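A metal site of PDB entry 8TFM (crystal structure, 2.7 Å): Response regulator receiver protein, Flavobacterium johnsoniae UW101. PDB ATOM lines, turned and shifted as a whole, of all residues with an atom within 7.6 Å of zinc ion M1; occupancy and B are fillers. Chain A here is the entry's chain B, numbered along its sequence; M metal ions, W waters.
OD1 of Asp 363 sits close to ND2 of Asn 241, at 3.4 Å. O of Asp 363 is in hydrogen-bond range of OG of Ser 366 (2.7 Å). O of His 502 lies within hydrogen-bond range of ND2 of Asn 438 (2.7 Å). ND1 of His 502 lies within hydrogen-bond range of O of Thr 272, 2.9 Å away.
Three residues have an atom within 4 Å of zinc ion M1: Asp 363, His 367 and His 502.
Zinc ion M1 is bound by the side-chain carboxylate of Asp 363 (2.0 Å), a ring nitrogen (NE2) of His 367 (2.2 Å), a ring nitrogen (NE2) of His 502 (2.3 Å) and water W1 (2.6 Å). Zinc ion M1 has four donor atoms within binding distance.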
ATOM      1  N   ASP A 240      32.443  28.749  14.259  1.00  0.00           N
ATOM      2  CA  ASP A 240      31.046  28.443  14.472  1.00  0.00           C
ATOM      3  C   ASP A 240      30.591  27.425  13.431  1.00  0.00           C
ATOM      4  O   ASP A 240      30.901  27.570  12.253  1.00  0.00           O
ATOM      5  CB  ASP A 240      30.183  29.698  14.401  1.00  0.00           C
ATOM      6  CG  ASP A 240      28.873  29.540  15.156  1.00  0.00           C
ATOM      7  OD1 ASP A 240      28.906  29.750  16.364  1.00  0.00           O
ATOM      8  OD2 ASP A 240      27.868  29.123  14.518  1.00  0.00           O
ATOM      9  N   ASN A 241      29.844  26.421  13.880  1.00  0.00           N
ATOM     10  CA  ASN A 241      29.065  25.559  13.017  1.00  0.00           C
ATOM     11  C   ASN A 241      29.989  24.747  12.101  1.00  0.00           C
ATOM     12  O   ASN A 241      29.787  24.728  10.890  1.00  0.00           O
ATOM     13  CB  ASN A 241      28.036  26.364  12.207  1.00  0.00           C
ATOM     14  CG  ASN A 241      27.066  25.482  11.431  1.00  0.00           C
ATOM     15  OD1 ASN A 241      27.158  24.265  11.473  1.00  0.00           O
ATOM     16  ND2 ASN A 241      26.155  26.087  10.677  1.00  0.00           N
ATOM     17  N   THR A 272      21.612  22.285  19.805  1.00  0.00           N
ATOM     18  CA  THR A 272      22.864  22.475  19.096  1.00  0.00           C
ATOM     19  C   THR A 272      22.817  23.803  18.320  1.00  0.00           C
ATOM     20  O   THR A 272      22.882  23.816  17.094  1.00  0.00           O
ATOM     21  CB  THR A 272      23.156  21.266  18.181  1.00  0.00           C
ATOM     22  OG1 THR A 272      22.001  20.970  17.397  1.00  0.00           O
ATOM     23  CG2 THR A 272      23.539  20.031  18.955  1.00  0.00           C
ATOM     24  N   ALA A 273      22.669  24.902  19.081  1.00  0.00           N
ATOM     25  CA  ALA A 273      22.595  26.245  18.526  1.00  0.00           C
ATOM     26  C   ALA A 273      23.558  27.179  19.265  1.00  0.00           C
ATOM     27  O   ALA A 273      23.853  26.969  20.455  1.00  0.00           O
ATOM     28  CB  ALA A 273      21.186  26.766  18.607  1.00  0.00           C
ATOM     29  N   THR A 274      24.019  28.206  18.538  1.00  0.00           N
ATOM     30  CA  THR A 274      25.009  29.163  19.022  1.00  0.00           C
ATOM     31  C   THR A 274      24.592  29.721  20.387  1.00  0.00           C
ATOM     32  O   THR A 274      25.403  29.723  21.319  1.00  0.00           O
ATOM     33  CB  THR A 274      25.248  30.259  17.971  1.00  0.00           C
ATOM     34  OG1 THR A 274      25.460  29.630  16.695  1.00  0.00           O
ATOM     35  CG2 THR A 274      26.420  31.164  18.315  1.00  0.00           C
ATOM     36  N   ASN A 360      32.512  33.441  12.449  1.00  0.00           N
ATOM     37  CA  ASN A 360      31.113  33.127  12.218  1.00  0.00           C
ATOM     38  C   ASN A 360      30.833  32.810  10.743  1.00  0.00           C
ATOM     39  O   ASN A 360      29.699  32.583  10.357  1.00  0.00           O
ATOM     40  CB  ASN A 360      30.214  34.279  12.652  1.00  0.00           C
ATOM     41  CG  ASN A 360      29.923  34.338  14.145  1.00  0.00           C
ATOM     42  OD1 ASN A 360      30.307  33.451  14.903  1.00  0.00           O
ATOM     43  ND2 ASN A 360      29.218  35.377  14.573  1.00  0.00           N
ATOM     44  N   VAL A 362      31.371  30.315   8.739  1.00  0.00           N
ATOM     45  CA  VAL A 362      30.905  29.041   8.212  1.00  0.00           C
ATOM     46  C   VAL A 362      29.401  28.922   8.462  1.00  0.00           C
ATOM     47  O   VAL A 362      28.673  28.366   7.639  1.00  0.00           O
ATOM     48  CB  VAL A 362      31.701  27.874   8.816  1.00  0.00           C
ATOM     49  CG1 VAL A 362      31.203  26.537   8.294  1.00  0.00           C
ATOM     50  CG2 VAL A 362      33.203  28.017   8.563  1.00  0.00           C
ATOM     51  N   ASP A 363      28.935  29.478   9.576  1.00  0.00           N
ATOM     52  CA  ASP A 363      27.513  29.506   9.871  1.00  0.00           C
ATOM     53  C   ASP A 363      26.777  30.327   8.826  1.00  0.00           C
ATOM     54  O   ASP A 363      25.746  29.894   8.330  1.00  0.00           O
ATOM     55  CB  ASP A 363      27.242  30.045  11.280  1.00  0.00           C
ATOM     56  CG  ASP A 363      25.759  30.146  11.557  1.00  0.00           C
ATOM     57  OD1 ASP A 363      25.116  29.082  11.784  1.00  0.00           O
ATOM     58  OD2 ASP A 363      25.237  31.293  11.485  1.00  0.00           O
ATOM     59  N   MET A 364      27.306  31.511   8.493  1.00  0.00           N
ATOM     60  CA  MET A 364      26.723  32.389   7.501  1.00  0.00           C
ATOM     61  C   MET A 364      26.618  31.636   6.177  1.00  0.00           C
ATOM     62  O   MET A 364      25.576  31.696   5.512  1.00  0.00           O
ATOM     63  CB  MET A 364      27.597  33.642   7.290  1.00  0.00           C
ATOM     64  CG  MET A 364      27.144  34.883   8.080  1.00  0.00           C
ATOM     65  SD  MET A 364      28.571  35.973   8.463  1.00  0.00           S
ATOM     66  CE  MET A 364      28.026  36.664  10.027  1.00  0.00           C
ATOM     67  N   SER A 366      26.653  28.291   5.631  1.00  0.00           N
ATOM     68  CA  SER A 366      25.740  27.163   5.706  1.00  0.00           C
ATOM     69  C   SER A 366      24.311  27.653   5.526  1.00  0.00           C
ATOM     70  O   SER A 366      23.546  27.020   4.796  1.00  0.00           O
ATOM     71  CB  SER A 366      25.891  26.393   6.998  1.00  0.00           C
ATOM     72  OG  SER A 366      25.511  27.176   8.111  1.00  0.00           O
ATOM     73  N   HIS A 367      23.981  28.784   6.171  1.00  0.00           N
ATOM     74  CA  HIS A 367      22.641  29.366   6.117  1.00  0.00           C
ATOM     75  C   HIS A 367      22.370  29.979   4.749  1.00  0.00           C
ATOM     76  O   HIS A 367      21.236  30.135   4.359  1.00  0.00           O
ATOM     77  CB  HIS A 367      22.436  30.359   7.266  1.00  0.00           C
ATOM     78  CG  HIS A 367      22.356  29.687   8.598  1.00  0.00           C
ATOM     79  ND1 HIS A 367      21.377  28.777   8.963  1.00  0.00           N
ATOM     80  CD2 HIS A 367      23.170  29.795   9.652  1.00  0.00           C
ATOM     81  CE1 HIS A 367      21.614  28.377  10.209  1.00  0.00           C
ATOM     82  NE2 HIS A 367      22.715  28.971  10.633  1.00  0.00           N
ATOM     83  N   ASP A 417      31.114  25.107  18.112  1.00  0.00           N
ATOM     84  CA  ASP A 417      30.015  25.069  19.063  1.00  0.00           C
ATOM     85  C   ASP A 417      29.118  23.872  18.757  1.00  0.00           C
ATOM     86  O   ASP A 417      28.569  23.279  19.693  1.00  0.00           O
ATOM     87  CB  ASP A 417      29.268  26.411  19.105  1.00  0.00           C
ATOM     88  CG  ASP A 417      28.718  26.918  17.778  1.00  0.00           C
ATOM     89  OD1 ASP A 417      29.201  26.431  16.713  1.00  0.00           O
ATOM     90  OD2 ASP A 417      27.791  27.785  17.828  1.00  0.00           O
ATOM     91  N   HIS A 418      28.995  23.522  17.464  1.00  0.00           N
ATOM     92  CA  HIS A 418      28.111  22.480  16.975  1.00  0.00           C
ATOM     93  C   HIS A 418      28.273  22.371  15.464  1.00  0.00           C
ATOM     94  O   HIS A 418      28.886  23.242  14.872  1.00  0.00           O
ATOM     95  CB  HIS A 418      26.637  22.819  17.243  1.00  0.00           C
ATOM     96  CG  HIS A 418      26.292  24.127  16.635  1.00  0.00           C
ATOM     97  ND1 HIS A 418      26.118  24.276  15.272  1.00  0.00           N
ATOM     98  CD2 HIS A 418      26.134  25.325  17.182  1.00  0.00           C
ATOM     99  CE1 HIS A 418      25.852  25.551  15.017  1.00  0.00           C
ATOM    100  NE2 HIS A 418      25.863  26.196  16.156  1.00  0.00           N
ATOM    101  N   GLY A 419      27.724  21.313  14.859  1.00  0.00           N
ATOM    102  CA  GLY A 419      27.718  21.136  13.411  1.00  0.00           C
ATOM    103  C   GLY A 419      26.377  21.530  12.823  1.00  0.00           C
ATOM    104  O   GLY A 419      25.574  22.170  13.496  1.00  0.00           O
ATOM    105  N   THR A 420      26.130  21.171  11.547  1.00  0.00           N
ATOM    106  CA  THR A 420      24.846  21.383  10.899  1.00  0.00           C
ATOM    107  C   THR A 420      24.535  20.143  10.043  1.00  0.00           C
ATOM    108  O   THR A 420      25.470  19.466   9.641  1.00  0.00           O
ATOM    109  CB  THR A 420      24.862  22.656  10.045  1.00  0.00           C
ATOM    110  OG1 THR A 420      23.558  22.829   9.484  1.00  0.00           O
ATOM    111  CG2 THR A 420      25.838  22.581   8.907  1.00  0.00           C
ATOM    112  N   ASN A 438      13.938  28.421  15.187  1.00  0.00           N
ATOM    113  CA  ASN A 438      14.812  27.459  14.518  1.00  0.00           C
ATOM    114  C   ASN A 438      13.967  26.409  13.782  1.00  0.00           C
ATOM    115  O   ASN A 438      12.745  26.502  13.750  1.00  0.00           O
ATOM    116  CB  ASN A 438      15.804  26.907  15.549  1.00  0.00           C
ATOM    117  CG  ASN A 438      16.772  25.898  14.949  1.00  0.00           C
ATOM    118  OD1 ASN A 438      17.268  26.091  13.842  1.00  0.00           O
ATOM    119  ND2 ASN A 438      16.981  24.771  15.616  1.00  0.00           N
ATOM    120  N   TYR A 500      20.975  23.449   5.296  1.00  0.00           N
ATOM    121  CA  TYR A 500      21.727  23.110   6.485  1.00  0.00           C
ATOM    122  C   TYR A 500      21.036  23.782   7.676  1.00  0.00           C
ATOM    123  O   TYR A 500      20.899  24.999   7.687  1.00  0.00           O
ATOM    124  CB  TYR A 500      23.214  23.478   6.299  1.00  0.00           C
ATOM    125  CG  TYR A 500      23.946  22.646   5.256  1.00  0.00           C
ATOM    126  CD1 TYR A 500      24.196  21.301   5.484  1.00  0.00           C
ATOM    127  CD2 TYR A 500      24.318  23.174   4.024  1.00  0.00           C
ATOM    128  CE1 TYR A 500      24.842  20.513   4.537  1.00  0.00           C
ATOM    129  CE2 TYR A 500      24.979  22.401   3.087  1.00  0.00           C
ATOM    130  CZ  TYR A 500      25.208  21.056   3.325  1.00  0.00           C
ATOM    131  OH  TYR A 500      25.833  20.219   2.429  1.00  0.00           O
ATOM    132  N   GLN A 501      20.567  22.988   8.650  1.00  0.00           N
ATOM    133  CA  GLN A 501      19.965  23.501   9.877  1.00  0.00           C
ATOM    134  C   GLN A 501      20.679  22.882  11.063  1.00  0.00           C
ATOM    135  O   GLN A 501      21.277  21.831  10.917  1.00  0.00           O
ATOM    136  CB  GLN A 501      18.499  23.099  10.022  1.00  0.00           C
ATOM    137  CG  GLN A 501      17.610  23.574   8.889  1.00  0.00           C
ATOM    138  CD  GLN A 501      17.644  25.073   8.733  1.00  0.00           C
ATOM    139  OE1 GLN A 501      17.716  25.820   9.708  1.00  0.00           O
ATOM    140  NE2 GLN A 501      17.579  25.511   7.481  1.00  0.00           N
ATOM    141  N   HIS A 502      20.602  23.507  12.246  1.00  0.00           N
ATOM    142  CA  HIS A 502      21.172  22.926  13.438  1.00  0.00           C
ATOM    143  C   HIS A 502      20.283  23.226  14.642  1.00  0.00           C
ATOM    144  O   HIS A 502      19.256  23.895  14.515  1.00  0.00           O
ATOM    145  CB  HIS A 502      22.610  23.406  13.624  1.00  0.00           C
ATOM    146  CG  HIS A 502      22.708  24.890  13.674  1.00  0.00           C
ATOM    147  ND1 HIS A 502      22.531  25.574  14.850  1.00  0.00           N
ATOM    148  CD2 HIS A 502      23.072  25.777  12.741  1.00  0.00           C
ATOM    149  CE1 HIS A 502      22.759  26.858  14.633  1.00  0.00           C
ATOM    150  NE2 HIS A 502      23.082  27.012  13.363  1.00  0.00           N
HETATM  151 ZN    ZN M   1      23.370  29.181  12.718  1.00  0.00          ZN
HETATM  152 ZN    ZN M   2      26.973  28.242  16.488  1.00  0.00          ZN
HETATM  153  O   HOH W   1      23.457  30.569  14.862  1.00  0.00           O
